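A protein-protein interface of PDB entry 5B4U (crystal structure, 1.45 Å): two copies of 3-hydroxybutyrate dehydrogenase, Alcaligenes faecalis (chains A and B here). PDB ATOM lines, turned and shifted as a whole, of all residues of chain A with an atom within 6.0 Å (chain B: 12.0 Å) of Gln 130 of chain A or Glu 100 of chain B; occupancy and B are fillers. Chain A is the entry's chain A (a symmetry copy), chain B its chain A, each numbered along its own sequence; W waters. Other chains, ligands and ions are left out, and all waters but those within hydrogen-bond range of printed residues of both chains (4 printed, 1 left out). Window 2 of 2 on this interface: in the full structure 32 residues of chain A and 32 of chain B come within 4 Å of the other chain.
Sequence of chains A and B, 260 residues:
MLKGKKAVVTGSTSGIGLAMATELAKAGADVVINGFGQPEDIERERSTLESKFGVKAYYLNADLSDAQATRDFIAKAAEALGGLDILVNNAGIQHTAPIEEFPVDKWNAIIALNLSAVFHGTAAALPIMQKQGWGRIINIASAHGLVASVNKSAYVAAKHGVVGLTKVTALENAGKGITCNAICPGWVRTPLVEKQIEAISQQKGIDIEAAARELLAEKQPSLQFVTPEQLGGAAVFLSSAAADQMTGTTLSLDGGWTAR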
ATOM      1  N   ARG A  71      -4.885 -11.867 -22.490  1.00  0.00           N
ATOM      2  CA  ARG A  71      -5.872 -12.434 -23.392  1.00  0.00           C
ATOM      3  C   ARG A  71      -6.458 -11.377 -24.332  1.00  0.00           C
ATOM      4  O   ARG A  71      -6.605 -11.618 -25.529  1.00  0.00           O
ATOM      5  CB  ARG A  71      -6.967 -13.133 -22.590  1.00  0.00           C
ATOM      6  CG  ARG A  71      -6.449 -14.392 -21.918  1.00  0.00           C
ATOM      7  CD  ARG A  71      -7.383 -14.920 -20.847  1.00  0.00           C
ATOM      8  NE  ARG A  71      -6.844 -16.125 -20.221  1.00  0.00           N
ATOM      9  CZ  ARG A  71      -7.123 -17.366 -20.608  1.00  0.00           C
ATOM     10  NH1 ARG A  71      -8.147 -17.605 -21.414  1.00  0.00           N
ATOM     11  NH2 ARG A  71      -6.452 -18.379 -20.088  1.00  0.00           N
ATOM     12  N   THR A 122      -1.059 -18.346 -24.870  1.00  0.00           N
ATOM     13  CA  THR A 122      -1.306 -19.583 -25.592  1.00  0.00           C
ATOM     14  C   THR A 122      -2.798 -19.898 -25.650  1.00  0.00           C
ATOM     15  O   THR A 122      -3.326 -20.250 -26.705  1.00  0.00           O
ATOM     16  CB  THR A 122      -0.538 -20.743 -24.937  1.00  0.00           C
ATOM     17  OG1 THR A 122       0.870 -20.486 -25.029  1.00  0.00           O
ATOM     18  CG2 THR A 122      -0.863 -22.067 -25.610  1.00  0.00           C
ATOM     19  N   ALA A 123      -3.479 -19.777 -24.514  1.00  0.00           N
ATOM     20  CA  ALA A 123      -4.911 -20.055 -24.461  1.00  0.00           C
ATOM     21  C   ALA A 123      -5.685 -19.179 -25.442  1.00  0.00           C
ATOM     22  O   ALA A 123      -6.651 -19.629 -26.064  1.00  0.00           O
ATOM     23  CB  ALA A 123      -5.436 -19.859 -23.047  1.00  0.00           C
ATOM     24  N   ALA A 124      -5.303 -17.911 -25.537  1.00  0.00           N
ATOM     25  CA  ALA A 124      -6.001 -16.977 -26.415  1.00  0.00           C
ATOM     26  C   ALA A 124      -5.687 -17.242 -27.885  1.00  0.00           C
ATOM     27  O   ALA A 124      -6.525 -17.012 -28.755  1.00  0.00           O
ATOM     28  CB  ALA A 124      -5.648 -15.543 -26.051  1.00  0.00           C
ATOM     29  N   ALA A 125      -4.452 -17.632 -28.177  1.00  0.00           N
ATOM     30  CA  ALA A 125      -4.029 -17.836 -29.558  1.00  0.00           C
ATOM     31  C   ALA A 125      -4.572 -19.134 -30.151  1.00  0.00           C
ATOM     32  O   ALA A 125      -4.767 -19.235 -31.362  1.00  0.00           O
ATOM     33  CB  ALA A 125      -2.513 -17.807 -29.658  1.00  0.00           C
ATOM     34  N   LEU A 126      -4.660 -20.176 -29.334  1.00  0.00           N
ATOM     35  CA  LEU A 126      -4.868 -21.520 -29.864  1.00  0.00           C
ATOM     36  C   LEU A 126      -6.127 -21.646 -30.721  1.00  0.00           C
ATOM     37  O   LEU A 126      -6.091 -22.300 -31.757  1.00  0.00           O
ATOM     38  CB  LEU A 126      -4.880 -22.558 -28.742  1.00  0.00           C
ATOM     39  CG  LEU A 126      -3.509 -23.101 -28.333  1.00  0.00           C
ATOM     40  CD1 LEU A 126      -3.620 -23.975 -27.095  1.00  0.00           C
ATOM     41  CD2 LEU A 126      -2.859 -23.864 -29.481  1.00  0.00           C
ATOM     42  N   PRO A 127      -7.242 -21.015 -30.308  1.00  0.00           N
ATOM     43  CA  PRO A 127      -8.452 -21.237 -31.102  1.00  0.00           C
ATOM     44  C   PRO A 127      -8.340 -20.679 -32.517  1.00  0.00           C
ATOM     45  O   PRO A 127      -8.832 -21.288 -33.468  1.00  0.00           O
ATOM     46  CB  PRO A 127      -9.530 -20.498 -30.308  1.00  0.00           C
ATOM     47  CG  PRO A 127      -9.044 -20.543 -28.900  1.00  0.00           C
ATOM     48  CD  PRO A 127      -7.549 -20.432 -28.989  1.00  0.00           C
ATOM     49  N   ILE A 128      -7.535 -19.636 -32.669  1.00  0.00           N
ATOM     50  CA  ILE A 128      -7.286 -19.038 -33.970  1.00  0.00           C
ATOM     51  C   ILE A 128      -6.462 -19.982 -34.839  1.00  0.00           C
ATOM     52  O   ILE A 128      -6.851 -20.317 -35.962  1.00  0.00           O
ATOM     53  CB  ILE A 128      -6.555 -17.695 -33.808  1.00  0.00           C
ATOM     54  CG1 ILE A 128      -7.417 -16.730 -32.988  1.00  0.00           C
ATOM     55  CG2 ILE A 128      -6.217 -17.101 -35.166  1.00  0.00           C
ATOM     56  CD1 ILE A 128      -6.678 -15.498 -32.515  1.00  0.00           C
ATOM     57  N   MET A 129      -5.424 -20.558 -34.247  1.00  0.00           N
ATOM     58  CA  MET A 129      -4.587 -21.514 -34.953  1.00  0.00           C
ATOM     59  C   MET A 129      -5.327 -22.815 -35.253  1.00  0.00           C
ATOM     60  O   MET A 129      -5.125 -23.420 -36.304  1.00  0.00           O
ATOM     61  CB  MET A 129      -3.331 -21.799 -34.138  1.00  0.00           C
ATOM     62  CG  MET A 129      -2.477 -20.570 -33.910  1.00  0.00           C
ATOM     63  SD  MET A 129      -1.083 -20.933 -32.834  1.00  0.00           S
ATOM     64  CE  MET A 129      -0.224 -19.362 -32.888  1.00  0.00           C
ATOM     65  N   GLN A 130      -6.173 -23.246 -34.325  1.00  0.00           N
ATOM     66  CA  GLN A 130      -6.909 -24.494 -34.484  1.00  0.00           C
ATOM     67  C   GLN A 130      -7.912 -24.402 -35.632  1.00  0.00           C
ATOM     68  O   GLN A 130      -8.021 -25.321 -36.444  1.00  0.00           O
ATOM     69  CB  GLN A 130      -7.618 -24.853 -33.177  1.00  0.00           C
ATOM     70  CG  GLN A 130      -6.667 -25.315 -32.081  1.00  0.00           C
ATOM     71  CD  GLN A 130      -7.305 -25.333 -30.705  1.00  0.00           C
ATOM     72  OE1 GLN A 130      -8.336 -24.699 -30.474  1.00  0.00           O
ATOM     73  NE2 GLN A 130      -6.641 -25.984 -29.758  1.00  0.00           N
ATOM     74  N   LYS A 131      -8.506 -23.227 -35.797  1.00  0.00           N
ATOM     75  CA  LYS A 131      -9.495 -23.015 -36.850  1.00  0.00           C
ATOM     76  C   LYS A 131      -8.848 -23.050 -38.230  1.00  0.00           C
ATOM     77  O   LYS A 131      -9.432 -23.568 -39.180  1.00  0.00           O
ATOM     78  CB  LYS A 131     -10.213 -21.681 -36.643  1.00  0.00           C
ATOM     79  CG  LYS A 131     -11.254 -21.368 -37.705  1.00  0.00           C
ATOM     80  CD  LYS A 131     -12.193 -20.262 -37.251  1.00  0.00           C
ATOM     81  CE  LYS A 131     -11.934 -18.967 -38.003  1.00  0.00           C
ATOM     82  NZ  LYS A 131     -12.824 -18.819 -39.188  1.00  0.00           N
ATOM     83  N   GLN A 132      -7.612 -22.577 -38.325  1.00  0.00           N
ATOM     84  CA  GLN A 132      -6.933 -22.506 -39.614  1.00  0.00           C
ATOM     85  C   GLN A 132      -6.075 -23.732 -39.901  1.00  0.00           C
ATOM     86  O   GLN A 132      -5.611 -23.914 -41.022  1.00  0.00           O
ATOM     87  CB  GLN A 132      -6.082 -21.247 -39.703  1.00  0.00           C
ATOM     88  CG  GLN A 132      -4.835 -21.275 -38.841  1.00  0.00           C
ATOM     89  CD  GLN A 132      -4.340 -19.882 -38.511  1.00  0.00           C
ATOM     90  OE1 GLN A 132      -3.333 -19.712 -37.818  1.00  0.00           O
ATOM     91  NE2 GLN A 132      -5.122 -18.879 -38.893  1.00  0.00           N
ATOM     92  N   GLY A 133      -5.822 -24.542 -38.879  1.00  0.00           N
ATOM     93  CA  GLY A 133      -5.058 -25.776 -39.056  1.00  0.00           C
ATOM     94  C   GLY A 133      -3.572 -25.553 -39.277  1.00  0.00           C
ATOM     95  O   GLY A 133      -2.891 -26.386 -39.867  1.00  0.00           O
ATOM     96  N   TRP A 134      -3.051 -24.458 -38.735  1.00  0.00           N
ATOM     97  CA  TRP A 134      -1.618 -24.190 -38.778  1.00  0.00           C
ATOM     98  C   TRP A 134      -1.275 -23.220 -37.668  1.00  0.00           C
ATOM     99  O   TRP A 134      -2.021 -22.280 -37.399  1.00  0.00           O
ATOM    100  CB  TRP A 134      -1.205 -23.587 -40.123  1.00  0.00           C
ATOM    101  CG  TRP A 134       0.277 -23.683 -40.402  1.00  0.00           C
ATOM    102  CD1 TRP A 134       0.914 -24.677 -41.090  1.00  0.00           C
ATOM    103  CD2 TRP A 134       1.300 -22.757 -40.003  1.00  0.00           C
ATOM    104  NE1 TRP A 134       2.263 -24.435 -41.134  1.00  0.00           N
ATOM    105  CE2 TRP A 134       2.529 -23.263 -40.475  1.00  0.00           C
ATOM    106  CE3 TRP A 134       1.298 -21.552 -39.291  1.00  0.00           C
ATOM    107  CZ2 TRP A 134       3.747 -22.639 -40.210  1.00  0.00           C
ATOM    108  CZ3 TRP A 134       2.512 -20.945 -39.015  1.00  0.00           C
ATOM    109  CH2 TRP A 134       3.710 -21.451 -39.535  1.00  0.00           C
ATOM    110  N   GLU A 172      -1.565 -31.548 -26.775  1.00  0.00           N
ATOM    111  CA  GLU A 172      -2.979 -31.250 -26.977  1.00  0.00           C
ATOM    112  C   GLU A 172      -3.280 -30.918 -28.430  1.00  0.00           C
ATOM    113  O   GLU A 172      -4.417 -31.059 -28.880  1.00  0.00           O
ATOM    114  CB  GLU A 172      -3.417 -30.089 -26.082  1.00  0.00           C
ATOM    115  CG  GLU A 172      -3.539 -30.470 -24.618  1.00  0.00           C
ATOM    116  CD  GLU A 172      -4.057 -29.345 -23.744  1.00  0.00           C
ATOM    117  OE1 GLU A 172      -4.491 -28.295 -24.280  1.00  0.00           O
ATOM    118  OE2 GLU A 172      -4.028 -29.517 -22.508  1.00  0.00           O
ATOM    119  N   ASN A 173      -2.265 -30.492 -29.170  1.00  0.00           N
ATOM    120  CA  ASN A 173      -2.470 -30.017 -30.533  1.00  0.00           C
ATOM    121  C   ASN A 173      -1.667 -30.829 -31.535  1.00  0.00           C
ATOM    122  O   ASN A 173      -1.595 -30.490 -32.717  1.00  0.00           O
ATOM    123  CB  ASN A 173      -2.124 -28.534 -30.624  1.00  0.00           C
ATOM    124  CG  ASN A 173      -3.104 -27.672 -29.860  1.00  0.00           C
ATOM    125  OD1 ASN A 173      -4.234 -27.479 -30.309  1.00  0.00           O
ATOM    126  ND2 ASN A 173      -2.781 -27.388 -28.609  1.00  0.00           N
ATOM    127  N   LYS A 176      -2.435 -31.376 -35.522  1.00  0.00           N
ATOM    128  CA  LYS A 176      -3.393 -30.355 -35.958  1.00  0.00           C
ATOM    129  C   LYS A 176      -2.761 -29.320 -36.886  1.00  0.00           C
ATOM    130  O   LYS A 176      -3.415 -28.347 -37.260  1.00  0.00           O
ATOM    131  CB  LYS A 176      -3.989 -29.625 -34.755  1.00  0.00           C
ATOM    132  CG  LYS A 176      -4.915 -30.460 -33.893  1.00  0.00           C
ATOM    133  CD  LYS A 176      -5.560 -29.596 -32.822  1.00  0.00           C
ATOM    134  CE  LYS A 176      -6.319 -30.427 -31.802  1.00  0.00           C
ATOM    135  NZ  LYS A 176      -6.772 -29.592 -30.657  1.00  0.00           N
ATOM    136  N   ILE A 178      -0.271 -27.510 -35.687  1.00  0.00           N
ATOM    137  CA  ILE A 178       0.233 -26.557 -34.706  1.00  0.00           C
ATOM    138  C   ILE A 178       1.352 -27.206 -33.912  1.00  0.00           C
ATOM    139  O   ILE A 178       1.168 -28.298 -33.374  1.00  0.00           O
ATOM    140  CB  ILE A 178      -0.872 -26.149 -33.716  1.00  0.00           C
ATOM    141  CG1 ILE A 178      -2.038 -25.504 -34.469  1.00  0.00           C
ATOM    142  CG2 ILE A 178      -0.320 -25.204 -32.661  1.00  0.00           C
ATOM    143  CD1 ILE A 178      -3.315 -25.417 -33.665  1.00  0.00           C
ATOM    144  N   HIS B  95      -6.874 -30.373 -11.871  1.00  0.00           N
ATOM    145  CA  HIS B  95      -8.036 -30.073 -12.697  1.00  0.00           C
ATOM    146  C   HIS B  95      -7.681 -30.334 -14.152  1.00  0.00           C
ATOM    147  O   HIS B  95      -6.619 -29.920 -14.605  1.00  0.00           O
ATOM    148  CB  HIS B  95      -8.426 -28.608 -12.537  1.00  0.00           C
ATOM    149  CG  HIS B  95      -9.636 -28.221 -13.324  1.00  0.00           C
ATOM    150  ND1 HIS B  95     -10.915 -28.446 -12.868  1.00  0.00           N
ATOM    151  CD2 HIS B  95      -9.763 -27.740 -14.582  1.00  0.00           C
ATOM    152  CE1 HIS B  95     -11.780 -28.063 -13.789  1.00  0.00           C
ATOM    153  NE2 HIS B  95     -11.107 -27.675 -14.856  1.00  0.00           N
ATOM    154  N   THR B  96      -8.546 -31.043 -14.872  1.00  0.00           N
ATOM    155  CA  THR B  96      -8.229 -31.446 -16.232  1.00  0.00           C
ATOM    156  C   THR B  96      -9.149 -30.775 -17.249  1.00  0.00           C
ATOM    157  O   THR B  96     -10.368 -30.725 -17.079  1.00  0.00           O
ATOM    158  CB  THR B  96      -8.278 -32.977 -16.400  1.00  0.00           C
ATOM    159  OG1 THR B  96      -9.638 -33.415 -16.470  1.00  0.00           O
ATOM    160  CG2 THR B  96      -7.586 -33.668 -15.232  1.00  0.00           C
ATOM    161  N   ALA B  97      -8.534 -30.139 -18.240  1.00  0.00           N
ATOM    162  CA  ALA B  97      -9.241 -29.466 -19.330  1.00  0.00           C
ATOM    163  C   ALA B  97      -8.203 -29.039 -20.361  1.00  0.00           C
ATOM    164  O   ALA B  97      -7.059 -28.770 -20.005  1.00  0.00           O
ATOM    165  CB  ALA B  97      -9.980 -28.247 -18.805  1.00  0.00           C
ATOM    166  N   PRO B  98      -8.601 -28.920 -21.634  1.00  0.00           N
ATOM    167  CA  PRO B  98      -7.648 -28.392 -22.599  1.00  0.00           C
ATOM    168  C   PRO B  98      -7.335 -26.921 -22.355  1.00  0.00           C
ATOM    169  O   PRO B  98      -8.096 -26.217 -21.689  1.00  0.00           O
ATOM    170  CB  PRO B  98      -8.361 -28.580 -23.935  1.00  0.00           C
ATOM    171  CG  PRO B  98      -9.810 -28.527 -23.598  1.00  0.00           C
ATOM    172  CD  PRO B  98      -9.957 -29.042 -22.194  1.00  0.00           C
ATOM    173  N   ILE B  99      -6.157 -26.499 -22.793  1.00  0.00           N
ATOM    174  CA  ILE B  99      -5.634 -25.185 -22.435  1.00  0.00           C
ATOM    175  C   ILE B  99      -6.641 -24.069 -22.729  1.00  0.00           C
ATOM    176  O   ILE B  99      -6.866 -23.195 -21.896  1.00  0.00           O
ATOM    177  CB  ILE B  99      -4.309 -24.895 -23.167  1.00  0.00           C
ATOM    178  CG1 ILE B  99      -3.176 -25.718 -22.548  1.00  0.00           C
ATOM    179  CG2 ILE B  99      -3.983 -23.413 -23.099  1.00  0.00           C
ATOM    180  CD1 ILE B  99      -1.988 -25.910 -23.466  1.00  0.00           C
ATOM    181  N   GLU B 100      -7.253 -24.101 -23.907  1.00  0.00           N
ATOM    182  CA  GLU B 100      -8.122 -23.012 -24.335  1.00  0.00           C
ATOM    183  C   GLU B 100      -9.443 -23.000 -23.564  1.00  0.00           C
ATOM    184  O   GLU B 100     -10.147 -21.987 -23.558  1.00  0.00           O
ATOM    185  CB  GLU B 100      -8.381 -23.095 -25.841  1.00  0.00           C
ATOM    186  CG  GLU B 100      -9.170 -24.315 -26.281  1.00  0.00           C
ATOM    187  CD  GLU B 100      -8.289 -25.494 -26.646  1.00  0.00           C
ATOM    188  OE1 GLU B 100      -7.109 -25.507 -26.241  1.00  0.00           O
ATOM    189  OE2 GLU B 100      -8.817 -26.469 -27.219  1.00  0.00           O
ATOM    190  N   GLU B 101      -9.692 -24.053 -22.788  1.00  0.00           N
ATOM    191  CA  GLU B 101     -10.881 -24.136 -21.951  1.00  0.00           C
ATOM    192  C   GLU B 101     -10.537 -24.092 -20.462  1.00  0.00           C
ATOM    193  O   GLU B 101     -11.411 -24.269 -19.618  1.00  0.00           O
ATOM    194  CB  GLU B 101     -11.649 -25.426 -22.252  1.00  0.00           C
ATOM    195  CG  GLU B 101     -12.308 -25.452 -23.619  1.00  0.00           C
ATOM    196  CD  GLU B 101     -13.243 -26.632 -23.784  1.00  0.00           C
ATOM    197  OE1 GLU B 101     -14.472 -26.430 -23.674  1.00  0.00           O
ATOM    198  OE2 GLU B 101     -12.747 -27.776 -23.778  1.00  0.00           O
ATOM    199  N   PHE B 102      -9.252 -24.011 -20.144  1.00  0.00           N
ATOM    200  CA  PHE B 102      -8.797 -24.233 -18.782  1.00  0.00           C
ATOM    201  C   PHE B 102      -9.117 -23.018 -17.921  1.00  0.00           C
ATOM    202  O   PHE B 102      -8.739 -21.904 -18.266  1.00  0.00           O
ATOM    203  CB  PHE B 102      -7.288 -24.490 -18.775  1.00  0.00           C
ATOM    204  CG  PHE B 102      -6.808 -25.235 -17.565  1.00  0.00           C
ATOM    205  CD1 PHE B 102      -6.647 -24.585 -16.352  1.00  0.00           C
ATOM    206  CD2 PHE B 102      -6.551 -26.590 -17.627  1.00  0.00           C
ATOM    207  CE1 PHE B 102      -6.257 -25.276 -15.224  1.00  0.00           C
ATOM    208  CE2 PHE B 102      -6.206 -27.292 -16.492  1.00  0.00           C
ATOM    209  CZ  PHE B 102      -6.001 -26.626 -15.301  1.00  0.00           C
ATOM    210  N   PRO B 103      -9.903 -23.209 -16.851  1.00  0.00           N
ATOM    211  CA  PRO B 103     -10.370 -22.028 -16.134  1.00  0.00           C
ATOM    212  C   PRO B 103      -9.217 -21.230 -15.529  1.00  0.00           C
ATOM    213  O   PRO B 103      -8.293 -21.805 -14.958  1.00  0.00           O
ATOM    214  CB  PRO B 103     -11.265 -22.610 -15.039  1.00  0.00           C
ATOM    215  CG  PRO B 103     -11.721 -23.922 -15.583  1.00  0.00           C
ATOM    216  CD  PRO B 103     -10.568 -24.440 -16.392  1.00  0.00           C
ATOM    217  N   VAL B 104      -9.231 -19.922 -15.740  1.00  0.00           N
ATOM    218  CA  VAL B 104      -8.187 -19.055 -15.223  1.00  0.00           C
ATOM    219  C   VAL B 104      -8.060 -19.188 -13.704  1.00  0.00           C
ATOM    220  O   VAL B 104      -6.951 -19.245 -13.166  1.00  0.00           O
ATOM    221  CB  VAL B 104      -8.448 -17.594 -15.624  1.00  0.00           C
ATOM    222  CG1 VAL B 104      -7.590 -16.644 -14.803  1.00  0.00           C
ATOM    223  CG2 VAL B 104      -8.196 -17.409 -17.113  1.00  0.00           C
ATOM    224  N   ASP B 105      -9.187 -19.325 -13.014  1.00  0.00           N
ATOM    225  CA  ASP B 105      -9.153 -19.493 -11.567  1.00  0.00           C
ATOM    226  C   ASP B 105      -8.527 -20.827 -11.157  1.00  0.00           C
ATOM    227  O   ASP B 105      -7.906 -20.923 -10.101  1.00  0.00           O
ATOM    228  CB  ASP B 105     -10.554 -19.353 -10.966  1.00  0.00           C
ATOM    229  CG  ASP B 105     -11.579 -20.184 -11.688  1.00  0.00           C
ATOM    230  OD1 ASP B 105     -11.936 -19.819 -12.831  1.00  0.00           O
ATOM    231  OD2 ASP B 105     -11.965 -21.239 -11.145  1.00  0.00           O
ATOM    232  N   LYS B 106      -8.695 -21.857 -11.982  1.00  0.00           N
ATOM    233  CA  LYS B 106      -8.080 -23.150 -11.703  1.00  0.00           C
ATOM    234  C   LYS B 106      -6.577 -23.122 -11.980  1.00  0.00           C
ATOM    235  O   LYS B 106      -5.795 -23.694 -11.230  1.00  0.00           O
ATOM    236  CB  LYS B 106      -8.751 -24.262 -12.511  1.00  0.00           C
ATOM    237  CG  LYS B 106     -10.147 -24.623 -12.023  1.00  0.00           C
ATOM    238  CD  LYS B 106     -10.092 -25.318 -10.674  1.00  0.00           C
ATOM    239  CE  LYS B 106     -11.481 -25.640 -10.157  1.00  0.00           C
ATOM    240  NZ  LYS B 106     -11.402 -26.381  -8.870  1.00  0.00           N
ATOM    241  N   TRP B 107      -6.167 -22.430 -13.037  1.00  0.00           N
ATOM    242  CA  TRP B 107      -4.743 -22.191 -13.249  1.00  0.00           C
ATOM    243  C   TRP B 107      -4.145 -21.506 -12.031  1.00  0.00           C
ATOM    244  O   TRP B 107      -3.177 -21.988 -11.458  1.00  0.00           O
ATOM    245  CB  TRP B 107      -4.505 -21.355 -14.509  1.00  0.00           C
ATOM    246  CG  TRP B 107      -3.101 -20.835 -14.636  1.00  0.00           C
ATOM    247  CD1 TRP B 107      -2.616 -19.673 -14.120  1.00  0.00           C
ATOM    248  CD2 TRP B 107      -1.996 -21.469 -15.298  1.00  0.00           C
ATOM    249  NE1 TRP B 107      -1.262 -19.585 -14.338  1.00  0.00           N
ATOM    250  CE2 TRP B 107      -0.856 -20.682 -15.049  1.00  0.00           C
ATOM    251  CE3 TRP B 107      -1.859 -22.629 -16.066  1.00  0.00           C
ATOM    252  CZ2 TRP B 107       0.406 -21.019 -15.536  1.00  0.00           C
ATOM    253  CZ3 TRP B 107      -0.595 -22.968 -16.534  1.00  0.00           C
ATOM    254  CH2 TRP B 107       0.516 -22.168 -16.260  1.00  0.00           C
ATOM    255  N   SER B 149       1.192 -34.688 -19.990  1.00  0.00           N
ATOM    256  CA  SER B 149       0.029 -35.334 -20.589  1.00  0.00           C
ATOM    257  C   SER B 149      -0.914 -34.243 -21.065  1.00  0.00           C
ATOM    258  O   SER B 149      -0.884 -33.126 -20.549  1.00  0.00           O
ATOM    259  CB  SER B 149      -0.704 -36.201 -19.564  1.00  0.00           C
ATOM    260  OG  SER B 149       0.088 -37.294 -19.140  1.00  0.00           O
ATOM    261  N   VAL B 150      -1.870 -34.616 -21.906  1.00  0.00           N
ATOM    262  CA  VAL B 150      -2.882 -33.673 -22.357  1.00  0.00           C
ATOM    263  C   VAL B 150      -3.785 -33.239 -21.211  1.00  0.00           C
ATOM    264  O   VAL B 150      -3.962 -33.956 -20.224  1.00  0.00           O
ATOM    265  CB  VAL B 150      -3.752 -34.253 -23.491  1.00  0.00           C
ATOM    266  CG1 VAL B 150      -2.907 -34.527 -24.726  1.00  0.00           C
ATOM    267  CG2 VAL B 150      -4.474 -35.513 -23.034  1.00  0.00           C
ATOM    268  N   ASN B 151      -4.257 -32.003 -21.310  1.00  0.00           N
ATOM    269  CA  ASN B 151      -5.331 -31.490 -20.469  1.00  0.00           C
ATOM    270  C   ASN B 151      -4.904 -31.271 -19.026  1.00  0.00           C
ATOM    271  O   ASN B 151      -5.737 -30.986 -18.171  1.00  0.00           O
ATOM    272  CB  ASN B 151      -6.561 -32.396 -20.537  1.00  0.00           C
ATOM    273  CG  ASN B 151      -7.162 -32.454 -21.926  1.00  0.00           C
ATOM    274  OD1 ASN B 151      -6.845 -31.630 -22.781  1.00  0.00           O
ATOM    275  ND2 ASN B 151      -7.867 -33.543 -22.213  1.00  0.00           N
ATOM    276  N   LYS B 152      -3.598 -31.123 -18.828  1.00  0.00           N
ATOM    277  CA  LYS B 152      -3.049 -30.867 -17.505  1.00  0.00           C
ATOM    278  C   LYS B 152      -2.027 -29.739 -17.521  1.00  0.00           C
ATOM    279  O   LYS B 152      -1.032 -29.778 -16.803  1.00  0.00           O
ATOM    280  CB  LYS B 152      -2.435 -32.149 -16.945  1.00  0.00           C
ATOM    281  CG  LYS B 152      -3.489 -33.184 -16.590  1.00  0.00           C
ATOM    282  CD  LYS B 152      -2.893 -34.464 -16.033  1.00  0.00           C
ATOM    283  CE  LYS B 152      -3.999 -35.410 -15.593  1.00  0.00           C
ATOM    284  NZ  LYS B 152      -3.472 -36.672 -15.009  1.00  0.00           N
ATOM    285  N   SER B 153      -2.329 -28.675 -18.257  1.00  0.00           N
ATOM    286  CA  SER B 153      -1.383 -27.577 -18.402  1.00  0.00           C
ATOM    287  C   SER B 153      -0.915 -27.028 -17.056  1.00  0.00           C
ATOM    288  O   SER B 153       0.285 -26.891 -16.813  1.00  0.00           O
ATOM    289  CB  SER B 153      -1.975 -26.458 -19.262  1.00  0.00           C
ATOM    290  OG  SER B 153      -3.243 -26.032 -18.784  1.00  0.00           O
ATOM    291  N   ALA B 154      -1.853 -26.617 -16.211  1.00  0.00           N
ATOM    292  CA  ALA B 154      -1.482 -25.986 -14.951  1.00  0.00           C
ATOM    293  C   ALA B 154      -0.664 -26.940 -14.081  1.00  0.00           C
ATOM    294  O   ALA B 154       0.298 -26.534 -13.429  1.00  0.00           O
ATOM    295  CB  ALA B 154      -2.725 -25.507 -14.210  1.00  0.00           C
HETATM  296  O   HOH W   1      -4.441 -28.134 -20.252  1.00  0.00           O
HETATM  297  O   HOH W   2      -7.805 -20.863 -20.579  1.00  0.00           O
HETATM  298  O   HOH W   3      -6.963 -28.848 -27.726  1.00  0.00           O
HETATM  299  O   HOH W   4      -5.131 -27.256 -26.734  1.00  0.00           O
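The backbone NH (N) of Ile 99 of chain B is in hydrogen-bond range of the side-chain carboxylate (OE1) of Glu 172 of chain A. The backbone NH (N) of Asn 151 of chain B is in hydrogen-bond range of the side-chain carboxylate (OE2) of Glu 172 of chain A, at 2.8 Å. OE2 of Glu 100 of chain B is in hydrogen-bond range of NE2 of Gln 130 of chain A (3.4 Å).
The side-chain amide nitrogen of Gln 130 of chain A sits at hydrogen-bond distance from the side-chain amide oxygen of Asn 173 of chain A (2.9 Å). NZ of Lys 176 of chain A lies within hydrogen-bond range of O of Glu 172 of chain A, 3.3 Å away. N of Ala 97 of chain B is in hydrogen-bond range of O of Asn 151 of chain B (2.9 Å).
Among the printed residues, pairs that only touch across the chains: Arg 71 of chain A with Val 104 of chain B (3.6 Å), Ala 123 of chain A with Ile 99 of chain B (3.7 Å), Ala 123 of chain A with Glu 100 of chain B (3.9 Å), Leu 126 of chain A with Glu 100 of chain B (3.9 Å), Glu 172 of chain A with Pro 98 of chain B (3.6 Å) and Glu 172 of chain A with Val 150 of chain B (3.9 Å).
Of chain B, only Glu 100 (3.4 Å) comes within 4 Å of Gln 130 of chain A. Glu 100 of chain B touches three residues of chain A. Of chain B, only Ile 99 and Glu 100 come within 4 Å of Ala 123 of chain A. Leu 126 of chain A touches just one residue of chain B: Glu 100 (3.9 Å). No residue of chain B comes within 4 Å of Pro 127 of chain A. No residue of chain B comes within 4 Å of Met 129 of chain A. No residue of chain B comes within 4 Å of Gln 132 of chain A. Of the printed residues of chain A, Ile 99 of chain B touches Ala 123 and Glu 172. Of the printed residues of chain B, Arg 71 of chain A touches Val 104. Of the printed residues of chain B, Glu 172 of chain A touches Pro 98, Ile 99, Val 150 and Asn 151. Ser 153 of chain B touches none of the printed residues of chain A. Glu 101 of chain B touches none of the printed residues of chain A. The nearest printed residue of chain B that does not touch Gln 130 of chain A is Pro 98 of chain B (6.6 Å). The nearest printed residue of chain B that does not touch Glu 172 of chain A is Ala 97 of chain B (4.001 Å).
Of the 18 printed residues of chain A, 5 touch a printed residue of chain B. Hydrophobic or aromatic side chains of chain B within 4 Å of the printed part of chain A: Pro 98, Ile 99, Val 104 and Val 150. Among the printed residues, no Asp or Glu carboxylate lies within 4 Å of a Lys or Arg side-chain nitrogen of the other chain.
No position is printed for both chains. Of the 9 pairs that touch across the chains among the printed residues, none has its exchanged pair printed and touching as well.
Water W4 lies within hydrogen-bond range of the side-chain carboxylate (OE1) of Glu 100 of chain B (2.7 Å), the side-chain carboxylate (OE1) of Glu 172 of chain A (2.7 Å) and the side-chain amide nitrogen (ND2) of Asn 173 of chain A (3.0 Å). Water W2 lies within hydrogen-bond range of the backbone carbonyl oxygen of Phe 102 of chain B (2.7 Å), the backbone carbonyl oxygen of Ile 99 of chain B (2.8 Å) and the guanidinium group of Arg 71 of chain A (2.9 Å). Water W3 bridges NZ of Lys 176 of chain A and OE2 of Glu 100 of chain B.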
